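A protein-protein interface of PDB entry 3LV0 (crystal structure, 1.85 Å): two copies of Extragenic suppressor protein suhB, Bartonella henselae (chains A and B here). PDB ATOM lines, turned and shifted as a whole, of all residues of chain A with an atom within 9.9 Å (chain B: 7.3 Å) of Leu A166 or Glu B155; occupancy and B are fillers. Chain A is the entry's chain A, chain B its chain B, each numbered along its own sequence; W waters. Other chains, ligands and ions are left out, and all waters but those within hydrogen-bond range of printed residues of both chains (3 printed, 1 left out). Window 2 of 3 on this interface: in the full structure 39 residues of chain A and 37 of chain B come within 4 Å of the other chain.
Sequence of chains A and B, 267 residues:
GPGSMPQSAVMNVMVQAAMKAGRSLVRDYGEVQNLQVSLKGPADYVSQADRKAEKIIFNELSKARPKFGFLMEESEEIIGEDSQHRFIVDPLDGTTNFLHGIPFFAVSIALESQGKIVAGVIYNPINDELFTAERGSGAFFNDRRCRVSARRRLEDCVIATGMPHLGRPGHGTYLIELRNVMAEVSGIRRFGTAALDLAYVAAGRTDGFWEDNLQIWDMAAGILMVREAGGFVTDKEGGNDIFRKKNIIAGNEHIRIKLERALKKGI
No position is printed for both chains.
Among the printed residues, pairs that only touch across the chains: Pro A164 with Met B182, His A100 with Arg B151, Leu A166 with Glu B184, Thr A96 with Val B158, His A100 with Val B158, His A171 with Met B182, Leu A166 with Ala B183, Leu A166 with Met B182, His A165 with Val B185, His A165 with Met B182, Ala A43 with Ser B186 and Leu A166 with Glu B155.
OG of Ser B186 is in hydrogen-bond range of OH of Tyr A45, at 2.9 Å.
The backbone NH (N) of Leu A166 lies within hydrogen-bond range of the backbone carbonyl oxygen (O) of Val B185 (3.4 Å).
The backbone carbonyl oxygen of Ser B186 lies within hydrogen-bond range of a ring nitrogen (NE2) of His A165, 3.1 Å away.
The backbone carbonyl oxygen of Cys B157 sits at hydrogen-bond distance from the backbone NH of Ser B186, 2.9 Å away.
NH1 of Arg B153 is in salt-bridge range of OE2 of Glu B155.
O of Asp B156 sits close to NE of Arg B151 (3.4 Å).
The backbone carbonyl oxygen (O) of His A165 is in hydrogen-bond range of a ring nitrogen (NE2) of His A171 (3.0 Å).
The backbone NH (N) of Glu B155 lies within hydrogen-bond range of the backbone carbonyl oxygen (O) of Glu B184 (3.1 Å).
The side-chain hydroxyl of Ser B186 lies within hydrogen-bond range of the backbone carbonyl oxygen of Glu B155 (2.6 Å).
Water W2 lies within hydrogen-bond range of a ring nitrogen (ND1) of His A100 (2.7 Å) and the guanidinium group (NH1) of Arg B151 (3.1 Å).
Water W3 lies within hydrogen-bond range of NE2 of His A100 (2.7 Å) and O of Asp B156 (2.8 Å).
Water W1 lies within hydrogen-bond range of the side-chain hydroxyl of Thr A96 (2.7 Å), the backbone carbonyl oxygen of Ala A43 (2.7 Å) and the backbone carbonyl oxygen of Ser B186 (2.8 Å).
Of the 16 printed residues of chain B, 8 touch a printed residue of chain A.
Printed residues of chain B that touch a printed residue of chain A: Arg B151, Glu B155, Val B158, Met B182, Ala B183, Glu B184, Val B185 and Ser B186.
Hydrophobic or aromatic side chains of chain B within 4 Å of the printed part of chain A: Val B158 and Met B182.
Of the 16 printed residues of chain A, 8 touch a printed residue of chain B.
Printed residues of chain A that touch a printed residue of chain B: Ala A43, Tyr A45, Thr A96, His A100, Pro A164, His A165, Leu A166 and His A171.
Among the printed residues, 15 pairs touch across the chains.
Among the printed residues, no Asp or Glu carboxylate lies within 4 Å of a Lys or Arg side-chain nitrogen of the other chain.
Pro A42 touches none of the printed residues of chain B.
Of the printed residues of chain B, Tyr A45 touches Ser B186 (2.9 Å).
Leu A166 touches just these residues of chain B: Glu B155, Met B182, Ala B183, Glu B184 and Val B185.
No residue of chain A comes within 4 Å of Arg B153.
Leu B154 touches none of the printed residues of chain A.
Of chain A, only Leu A166 comes within 4 Å of Glu B155.
No residue of chain A comes within 4 Å of Asp B156.
No residue of chain A comes within 4 Å of Cys B157.
Of the printed residues of chain A, Val B158 touches Thr A96 and His A100.
Printed residues of chain A within 4 Å of Ala B183: Leu A166.
Gly B187 touches none of the printed residues of chain A.
The nearest residue of chain B that does not touch Leu A166 is Ser B186 (4.7 Å).
The nearest printed residue of chain A that does not touch Ala B183 is His A171 (4.001 Å).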
ATOM      1  N   LEU A  39     -21.315  14.523 -18.845  1.00  0.00           N
ATOM      2  CA  LEU A  39     -20.053  15.225 -19.001  1.00  0.00           C
ATOM      3  C   LEU A  39     -19.021  14.578 -18.110  1.00  0.00           C
ATOM      4  O   LEU A  39     -19.277  14.355 -16.924  1.00  0.00           O
ATOM      5  CB  LEU A  39     -20.200  16.694 -18.602  1.00  0.00           C
ATOM      6  CG  LEU A  39     -20.824  17.667 -19.590  1.00  0.00           C
ATOM      7  CD1 LEU A  39     -21.290  18.920 -18.844  1.00  0.00           C
ATOM      8  CD2 LEU A  39     -19.814  18.000 -20.674  1.00  0.00           C
ATOM      9  N   GLY A  41     -16.005  16.142 -18.211  1.00  0.00           N
ATOM     10  CA  GLY A  41     -15.278  17.387 -17.968  1.00  0.00           C
ATOM     11  C   GLY A  41     -15.907  18.444 -18.865  1.00  0.00           C
ATOM     12  O   GLY A  41     -16.769  18.113 -19.686  1.00  0.00           O
ATOM     13  N   PRO A  42     -15.513  19.725 -18.708  1.00  0.00           N
ATOM     14  CA  PRO A  42     -16.084  20.743 -19.602  1.00  0.00           C
ATOM     15  C   PRO A  42     -15.997  20.290 -21.082  1.00  0.00           C
ATOM     16  O   PRO A  42     -14.919  19.908 -21.548  1.00  0.00           O
ATOM     17  CB  PRO A  42     -15.207  21.973 -19.330  1.00  0.00           C
ATOM     18  CG  PRO A  42     -14.792  21.808 -17.880  1.00  0.00           C
ATOM     19  CD  PRO A  42     -14.660  20.317 -17.654  1.00  0.00           C
ATOM     20  N   ALA A  43     -17.139  20.283 -21.779  1.00  0.00           N
ATOM     21  CA  ALA A  43     -17.232  19.886 -23.210  1.00  0.00           C
ATOM     22  C   ALA A  43     -16.694  18.483 -23.539  1.00  0.00           C
ATOM     23  O   ALA A  43     -16.260  18.211 -24.662  1.00  0.00           O
ATOM     24  CB  ALA A  43     -16.581  20.940 -24.124  1.00  0.00           C
ATOM     25  N   ASP A  44     -16.746  17.579 -22.571  1.00  0.00           N
ATOM     26  CA  ASP A  44     -16.145  16.265 -22.768  1.00  0.00           C
ATOM     27  C   ASP A  44     -17.210  15.234 -22.409  1.00  0.00           C
ATOM     28  O   ASP A  44     -17.485  15.001 -21.226  1.00  0.00           O
ATOM     29  CB  ASP A  44     -14.864  16.151 -21.921  1.00  0.00           C
ATOM     30  CG  ASP A  44     -14.108  14.845 -22.153  1.00  0.00           C
ATOM     31  OD1 ASP A  44     -14.402  14.103 -23.115  1.00  0.00           O
ATOM     32  OD2 ASP A  44     -13.213  14.558 -21.337  1.00  0.00           O
ATOM     33  N   TYR A  45     -17.841  14.681 -23.451  1.00  0.00           N
ATOM     34  CA  TYR A  45     -19.070  13.882 -23.328  1.00  0.00           C
ATOM     35  C   TYR A  45     -18.792  12.391 -23.448  1.00  0.00           C
ATOM     36  O   TYR A  45     -17.851  11.977 -24.120  1.00  0.00           O
ATOM     37  CB  TYR A  45     -20.082  14.292 -24.415  1.00  0.00           C
ATOM     38  CG  TYR A  45     -20.462  15.760 -24.341  1.00  0.00           C
ATOM     39  CD1 TYR A  45     -21.482  16.199 -23.492  1.00  0.00           C
ATOM     40  CD2 TYR A  45     -19.780  16.716 -25.105  1.00  0.00           C
ATOM     41  CE1 TYR A  45     -21.813  17.568 -23.411  1.00  0.00           C
ATOM     42  CE2 TYR A  45     -20.095  18.070 -25.028  1.00  0.00           C
ATOM     43  CZ  TYR A  45     -21.111  18.490 -24.190  1.00  0.00           C
ATOM     44  OH  TYR A  45     -21.407  19.834 -24.131  1.00  0.00           O
ATOM     45  N   THR A  96     -18.635  14.012 -29.644  1.00  0.00           N
ATOM     46  CA  THR A  96     -19.411  15.221 -29.905  1.00  0.00           C
ATOM     47  C   THR A  96     -20.063  15.186 -31.325  1.00  0.00           C
ATOM     48  O   THR A  96     -21.242  15.449 -31.480  1.00  0.00           O
ATOM     49  CB  THR A  96     -18.538  16.462 -29.683  1.00  0.00           C
ATOM     50  OG1 THR A  96     -18.174  16.497 -28.295  1.00  0.00           O
ATOM     51  CG2 THR A  96     -19.308  17.778 -30.065  1.00  0.00           C
ATOM     52  N   HIS A 100     -24.241  14.970 -32.271  1.00  0.00           N
ATOM     53  CA  HIS A 100     -24.803  16.001 -33.139  1.00  0.00           C
ATOM     54  C   HIS A 100     -25.262  15.490 -34.523  1.00  0.00           C
ATOM     55  O   HIS A 100     -25.734  16.284 -35.338  1.00  0.00           O
ATOM     56  CB  HIS A 100     -23.766  17.133 -33.321  1.00  0.00           C
ATOM     57  CG  HIS A 100     -23.726  18.091 -32.170  1.00  0.00           C
ATOM     58  ND1 HIS A 100     -24.255  19.362 -32.236  1.00  0.00           N
ATOM     59  CD2 HIS A 100     -23.222  17.956 -30.922  1.00  0.00           C
ATOM     60  CE1 HIS A 100     -24.106  19.962 -31.067  1.00  0.00           C
ATOM     61  NE2 HIS A 100     -23.482  19.129 -30.250  1.00  0.00           N
ATOM     62  N   MET A 163      -8.409  21.297 -31.986  1.00  0.00           N
ATOM     63  CA  MET A 163      -8.370  22.539 -31.222  1.00  0.00           C
ATOM     64  C   MET A 163      -8.562  22.323 -29.730  1.00  0.00           C
ATOM     65  O   MET A 163      -9.130  21.309 -29.307  1.00  0.00           O
ATOM     66  CB  MET A 163      -9.446  23.493 -31.729  1.00  0.00           C
ATOM     67  CG  MET A 163      -9.317  23.844 -33.192  1.00  0.00           C
ATOM     68  SD  MET A 163     -10.639  24.955 -33.673  1.00  0.00           S
ATOM     69  CE  MET A 163     -10.230  25.310 -35.389  1.00  0.00           C
ATOM     70  N   PRO A 164      -8.058  23.261 -28.916  1.00  0.00           N
ATOM     71  CA  PRO A 164      -8.651  23.334 -27.596  1.00  0.00           C
ATOM     72  C   PRO A 164      -9.975  24.090 -27.747  1.00  0.00           C
ATOM     73  O   PRO A 164     -10.154  24.879 -28.682  1.00  0.00           O
ATOM     74  CB  PRO A 164      -7.630  24.154 -26.792  1.00  0.00           C
ATOM     75  CG  PRO A 164      -6.896  24.961 -27.805  1.00  0.00           C
ATOM     76  CD  PRO A 164      -6.899  24.164 -29.075  1.00  0.00           C
ATOM     77  N   HIS A 165     -10.922  23.822 -26.874  1.00  0.00           N
ATOM     78  CA  HIS A 165     -12.087  24.696 -26.770  1.00  0.00           C
ATOM     79  C   HIS A 165     -12.374  24.858 -25.290  1.00  0.00           C
ATOM     80  O   HIS A 165     -11.468  24.669 -24.470  1.00  0.00           O
ATOM     81  CB  HIS A 165     -13.289  24.174 -27.586  1.00  0.00           C
ATOM     82  CG  HIS A 165     -13.522  22.703 -27.443  1.00  0.00           C
ATOM     83  ND1 HIS A 165     -13.289  21.809 -28.469  1.00  0.00           N
ATOM     84  CD2 HIS A 165     -13.930  21.966 -26.382  1.00  0.00           C
ATOM     85  CE1 HIS A 165     -13.552  20.584 -28.048  1.00  0.00           C
ATOM     86  NE2 HIS A 165     -13.948  20.652 -26.786  1.00  0.00           N
ATOM     87  N   LEU A 166     -13.620  25.207 -24.975  1.00  0.00           N
ATOM     88  CA  LEU A 166     -14.094  25.572 -23.631  1.00  0.00           C
ATOM     89  C   LEU A 166     -13.103  25.415 -22.449  1.00  0.00           C
ATOM     90  O   LEU A 166     -12.855  24.312 -21.959  1.00  0.00           O
ATOM     91  CB  LEU A 166     -15.430  24.865 -23.347  1.00  0.00           C
ATOM     92  CG  LEU A 166     -16.479  25.559 -22.482  1.00  0.00           C
ATOM     93  CD1 LEU A 166     -16.856  26.916 -23.034  1.00  0.00           C
ATOM     94  CD2 LEU A 166     -17.716  24.682 -22.371  1.00  0.00           C
ATOM     95  N   PRO A 169      -7.592  25.687 -22.180  1.00  0.00           N
ATOM     96  CA  PRO A 169      -6.143  25.904 -21.981  1.00  0.00           C
ATOM     97  C   PRO A 169      -5.279  25.809 -23.270  1.00  0.00           C
ATOM     98  O   PRO A 169      -5.472  24.934 -24.092  1.00  0.00           O
ATOM     99  CB  PRO A 169      -5.783  24.841 -20.943  1.00  0.00           C
ATOM    100  CG  PRO A 169      -7.038  24.818 -20.052  1.00  0.00           C
ATOM    101  CD  PRO A 169      -8.230  25.119 -20.972  1.00  0.00           C
ATOM    102  N   GLY A 170      -4.363  26.764 -23.449  1.00  0.00           N
ATOM    103  CA  GLY A 170      -3.528  26.799 -24.647  1.00  0.00           C
ATOM    104  C   GLY A 170      -4.133  27.442 -25.891  1.00  0.00           C
ATOM    105  O   GLY A 170      -3.609  27.256 -26.992  1.00  0.00           O
ATOM    106  N   HIS A 171      -5.225  28.198 -25.734  1.00  0.00           N
ATOM    107  CA  HIS A 171      -5.909  28.793 -26.901  1.00  0.00           C
ATOM    108  C   HIS A 171      -5.011  29.797 -27.640  1.00  0.00           C
ATOM    109  O   HIS A 171      -4.980  29.839 -28.864  1.00  0.00           O
ATOM    110  CB  HIS A 171      -7.217  29.477 -26.473  1.00  0.00           C
ATOM    111  CG  HIS A 171      -8.314  28.519 -26.114  1.00  0.00           C
ATOM    112  ND1 HIS A 171      -9.640  28.755 -26.415  1.00  0.00           N
ATOM    113  CD2 HIS A 171      -8.283  27.326 -25.471  1.00  0.00           C
ATOM    114  CE1 HIS A 171     -10.377  27.753 -25.968  1.00  0.00           C
ATOM    115  NE2 HIS A 171      -9.578  26.873 -25.388  1.00  0.00           N
ATOM    116  N   ARG A 190     -11.025  20.940 -39.687  1.00  0.00           N
ATOM    117  CA  ARG A 190     -11.173  20.532 -38.288  1.00  0.00           C
ATOM    118  C   ARG A 190     -12.411  19.650 -38.225  1.00  0.00           C
ATOM    119  O   ARG A 190     -13.535  20.139 -38.132  1.00  0.00           O
ATOM    120  CB  ARG A 190     -11.290  21.754 -37.374  1.00  0.00           C
ATOM    121  CG  ARG A 190     -11.033  21.468 -35.864  1.00  0.00           C
ATOM    122  CD  ARG A 190     -12.057  20.506 -35.282  1.00  0.00           C
ATOM    123  NE  ARG A 190     -12.033  20.508 -33.812  1.00  0.00           N
ATOM    124  CZ  ARG A 190     -11.407  19.606 -33.072  1.00  0.00           C
ATOM    125  NH1 ARG A 190     -10.736  18.598 -33.645  1.00  0.00           N
ATOM    126  NH2 ARG A 190     -11.461  19.712 -31.748  1.00  0.00           N
ATOM    127  N   ARG B 151     -30.689  24.820 -28.963  1.00  0.00           N
ATOM    128  CA  ARG B 151     -29.724  25.196 -27.921  1.00  0.00           C
ATOM    129  C   ARG B 151     -29.745  26.698 -27.702  1.00  0.00           C
ATOM    130  O   ARG B 151     -29.999  27.473 -28.636  1.00  0.00           O
ATOM    131  CB  ARG B 151     -28.318  24.698 -28.274  1.00  0.00           C
ATOM    132  CG  ARG B 151     -28.236  23.164 -28.238  1.00  0.00           C
ATOM    133  CD  ARG B 151     -26.806  22.643 -28.446  1.00  0.00           C
ATOM    134  NE  ARG B 151     -26.773  21.177 -28.339  1.00  0.00           N
ATOM    135  CZ  ARG B 151     -27.028  20.327 -29.336  1.00  0.00           C
ATOM    136  NH1 ARG B 151     -27.322  20.755 -30.554  1.00  0.00           N
ATOM    137  NH2 ARG B 151     -26.990  19.023 -29.110  1.00  0.00           N
ATOM    138  N   ARG B 152     -29.522  27.109 -26.460  1.00  0.00           N
ATOM    139  CA  ARG B 152     -29.571  28.520 -26.137  1.00  0.00           C
ATOM    140  C   ARG B 152     -28.252  29.033 -25.608  1.00  0.00           C
ATOM    141  O   ARG B 152     -28.032  30.239 -25.589  1.00  0.00           O
ATOM    142  CB  ARG B 152     -30.657  28.786 -25.108  1.00  0.00           C
ATOM    143  CG  ARG B 152     -32.035  28.841 -25.692  1.00  0.00           C
ATOM    144  CD  ARG B 152     -32.907  29.576 -24.708  1.00  0.00           C
ATOM    145  NE  ARG B 152     -34.266  29.748 -25.197  1.00  0.00           N
ATOM    146  CZ  ARG B 152     -35.259  30.236 -24.465  1.00  0.00           C
ATOM    147  NH1 ARG B 152     -36.466  30.362 -24.991  1.00  0.00           N
ATOM    148  NH2 ARG B 152     -35.044  30.597 -23.207  1.00  0.00           N
ATOM    149  N   ARG B 153     -27.391  28.138 -25.146  1.00  0.00           N
ATOM    150  CA  ARG B 153     -26.110  28.570 -24.575  1.00  0.00           C
ATOM    151  C   ARG B 153     -24.979  28.120 -25.476  1.00  0.00           C
ATOM    152  O   ARG B 153     -24.916  26.950 -25.855  1.00  0.00           O
ATOM    153  CB  ARG B 153     -25.868  27.992 -23.181  1.00  0.00           C
ATOM    154  CG  ARG B 153     -27.051  28.070 -22.189  1.00  0.00           C
ATOM    155  CD  ARG B 153     -26.640  27.484 -20.838  1.00  0.00           C
ATOM    156  NE  ARG B 153     -26.080  26.135 -20.986  1.00  0.00           N
ATOM    157  CZ  ARG B 153     -25.475  25.445 -20.017  1.00  0.00           C
ATOM    158  NH1 ARG B 153     -25.339  25.963 -18.795  1.00  0.00           N
ATOM    159  NH2 ARG B 153     -24.995  24.231 -20.266  1.00  0.00           N
ATOM    160  N   LEU B 154     -24.054  29.031 -25.755  1.00  0.00           N
ATOM    161  CA  LEU B 154     -22.878  28.706 -26.563  1.00  0.00           C
ATOM    162  C   LEU B 154     -22.035  27.557 -26.003  1.00  0.00           C
ATOM    163  O   LEU B 154     -21.464  26.803 -26.772  1.00  0.00           O
ATOM    164  CB  LEU B 154     -21.987  29.942 -26.761  1.00  0.00           C
ATOM    165  CG  LEU B 154     -22.411  31.020 -27.775  1.00  0.00           C
ATOM    166  CD1 LEU B 154     -21.370  32.093 -27.780  1.00  0.00           C
ATOM    167  CD2 LEU B 154     -22.625  30.489 -29.219  1.00  0.00           C
ATOM    168  N   GLU B 155     -21.973  27.417 -24.674  1.00  0.00           N
ATOM    169  CA  GLU B 155     -21.175  26.336 -24.055  1.00  0.00           C
ATOM    170  C   GLU B 155     -21.665  24.927 -24.427  1.00  0.00           C
ATOM    171  O   GLU B 155     -20.910  23.969 -24.349  1.00  0.00           O
ATOM    172  CB  GLU B 155     -21.066  26.515 -22.526  1.00  0.00           C
ATOM    173  CG  GLU B 155     -22.365  26.227 -21.781  1.00  0.00           C
ATOM    174  CD  GLU B 155     -22.247  26.511 -20.296  1.00  0.00           C
ATOM    175  OE1 GLU B 155     -21.277  26.056 -19.662  1.00  0.00           O
ATOM    176  OE2 GLU B 155     -23.125  27.194 -19.766  1.00  0.00           O
ATOM    177  N   ASP B 156     -22.907  24.816 -24.885  1.00  0.00           N
ATOM    178  CA  ASP B 156     -23.455  23.533 -25.338  1.00  0.00           C
ATOM    179  C   ASP B 156     -23.296  23.318 -26.856  1.00  0.00           C
ATOM    180  O   ASP B 156     -23.665  22.262 -27.382  1.00  0.00           O
ATOM    181  CB  ASP B 156     -24.941  23.449 -24.981  1.00  0.00           C
ATOM    182  CG  ASP B 156     -25.185  23.655 -23.490  1.00  0.00           C
ATOM    183  OD1 ASP B 156     -24.422  23.079 -22.685  1.00  0.00           O
ATOM    184  OD2 ASP B 156     -26.110  24.409 -23.135  1.00  0.00           O
ATOM    185  N   CYS B 157     -22.777  24.317 -27.560  1.00  0.00           N
ATOM    186  CA  CYS B 157     -22.884  24.346 -29.027  1.00  0.00           C
ATOM    187  C   CYS B 157     -21.663  23.842 -29.770  1.00  0.00           C
ATOM    188  O   CYS B 157     -20.535  23.991 -29.314  1.00  0.00           O
ATOM    189  CB  CYS B 157     -23.110  25.785 -29.514  1.00  0.00           C
ATOM    190  SG  CYS B 157     -24.790  26.385 -29.208  1.00  0.00           S
ATOM    191  N   VAL B 158     -21.911  23.318 -30.958  1.00  0.00           N
ATOM    192  CA  VAL B 158     -20.880  23.110 -31.945  1.00  0.00           C
ATOM    193  C   VAL B 158     -21.100  24.114 -33.087  1.00  0.00           C
ATOM    194  O   VAL B 158     -22.187  24.160 -33.685  1.00  0.00           O
ATOM    195  CB  VAL B 158     -20.928  21.689 -32.501  1.00  0.00           C
ATOM    196  CG1 VAL B 158     -19.953  21.558 -33.728  1.00  0.00           C
ATOM    197  CG2 VAL B 158     -20.572  20.676 -31.380  1.00  0.00           C
ATOM    198  N   VAL B 181     -15.113  32.895 -30.324  1.00  0.00           N
ATOM    199  CA  VAL B 181     -16.055  31.779 -30.389  1.00  0.00           C
ATOM    200  C   VAL B 181     -15.462  30.541 -29.692  1.00  0.00           C
ATOM    201  O   VAL B 181     -16.134  29.924 -28.859  1.00  0.00           O
ATOM    202  CB  VAL B 181     -16.465  31.485 -31.857  1.00  0.00           C
ATOM    203  CG1 VAL B 181     -17.518  30.326 -31.930  1.00  0.00           C
ATOM    204  CG2 VAL B 181     -17.088  32.731 -32.474  1.00  0.00           C
ATOM    205  N   MET B 182     -14.204  30.215 -29.984  1.00  0.00           N
ATOM    206  CA  MET B 182     -13.522  29.042 -29.383  1.00  0.00           C
ATOM    207  C   MET B 182     -13.552  29.027 -27.880  1.00  0.00           C
ATOM    208  O   MET B 182     -13.609  27.961 -27.271  1.00  0.00           O
ATOM    209  CB  MET B 182     -12.020  29.023 -29.704  1.00  0.00           C
ATOM    210  CG  MET B 182     -11.641  28.569 -31.030  1.00  0.00           C
ATOM    211  SD  MET B 182      -9.816  28.774 -31.034  1.00  0.00           S
ATOM    212  CE  MET B 182      -9.328  27.231 -30.304  1.00  0.00           C
ATOM    213  N   ALA B 183     -13.478  30.205 -27.270  1.00  0.00           N
ATOM    214  CA  ALA B 183     -13.467  30.290 -25.818  1.00  0.00           C
ATOM    215  C   ALA B 183     -14.800  29.914 -25.179  1.00  0.00           C
ATOM    216  O   ALA B 183     -14.849  29.651 -23.976  1.00  0.00           O
ATOM    217  CB  ALA B 183     -13.032  31.696 -25.365  1.00  0.00           C
ATOM    218  N   GLU B 184     -15.874  29.875 -25.977  1.00  0.00           N
ATOM    219  CA  GLU B 184     -17.230  29.803 -25.430  1.00  0.00           C
ATOM    220  C   GLU B 184     -18.006  28.524 -25.771  1.00  0.00           C
ATOM    221  O   GLU B 184     -19.058  28.298 -25.188  1.00  0.00           O
ATOM    222  CB  GLU B 184     -18.073  30.986 -25.928  1.00  0.00           C
ATOM    223  CG  GLU B 184     -17.506  32.367 -25.670  1.00  0.00           C
ATOM    224  CD  GLU B 184     -17.398  32.722 -24.200  1.00  0.00           C
ATOM    225  OE1 GLU B 184     -18.096  32.113 -23.355  1.00  0.00           O
ATOM    226  OE2 GLU B 184     -16.584  33.616 -23.880  1.00  0.00           O
ATOM    227  N   VAL B 185     -17.523  27.732 -26.721  1.00  0.00           N
ATOM    228  CA  VAL B 185     -18.345  26.625 -27.275  1.00  0.00           C
ATOM    229  C   VAL B 185     -17.817  25.217 -26.947  1.00  0.00           C
ATOM    230  O   VAL B 185     -16.657  25.070 -26.572  1.00  0.00           O
ATOM    231  CB  VAL B 185     -18.507  26.784 -28.833  1.00  0.00           C
ATOM    232  CG1 VAL B 185     -19.228  28.077 -29.172  1.00  0.00           C
ATOM    233  CG2 VAL B 185     -17.119  26.704 -29.518  1.00  0.00           C
ATOM    234  N   SER B 186     -18.654  24.186 -27.129  1.00  0.00           N
ATOM    235  CA  SER B 186     -18.214  22.797 -26.997  1.00  0.00           C
ATOM    236  C   SER B 186     -17.400  22.324 -28.213  1.00  0.00           C
ATOM    237  O   SER B 186     -16.708  21.302 -28.148  1.00  0.00           O
ATOM    238  CB  SER B 186     -19.401  21.849 -26.835  1.00  0.00           C
ATOM    239  OG  SER B 186     -19.846  21.847 -25.501  1.00  0.00           O
ATOM    240  N   GLY B 187     -17.501  23.017 -29.331  1.00  0.00           N
ATOM    241  CA  GLY B 187     -16.678  22.608 -30.453  1.00  0.00           C
ATOM    242  C   GLY B 187     -16.716  23.572 -31.593  1.00  0.00           C
ATOM    243  O   GLY B 187     -17.709  24.235 -31.808  1.00  0.00           O
ATOM    244  N   ILE B 255     -28.691  31.536 -30.737  1.00  0.00           N
ATOM    245  CA  ILE B 255     -27.292  31.313 -31.077  1.00  0.00           C
ATOM    246  C   ILE B 255     -26.782  32.321 -32.123  1.00  0.00           C
ATOM    247  O   ILE B 255     -25.649  32.766 -32.021  1.00  0.00           O
ATOM    248  CB  ILE B 255     -27.035  29.859 -31.524  1.00  0.00           C
ATOM    249  CG1 ILE B 255     -27.468  28.852 -30.437  1.00  0.00           C
ATOM    250  CG2 ILE B 255     -25.556  29.663 -31.934  1.00  0.00           C
ATOM    251  CD1 ILE B 255     -26.853  29.080 -29.009  1.00  0.00           C
HETATM  252  O   HOH W   1     -17.088  18.723 -27.216  1.00  0.00           O
HETATM  253  O   HOH W   2     -26.124  20.895 -33.412  1.00  0.00           O
HETATM  254  O   HOH W   3     -22.635  19.701 -27.757  1.00  0.00           O
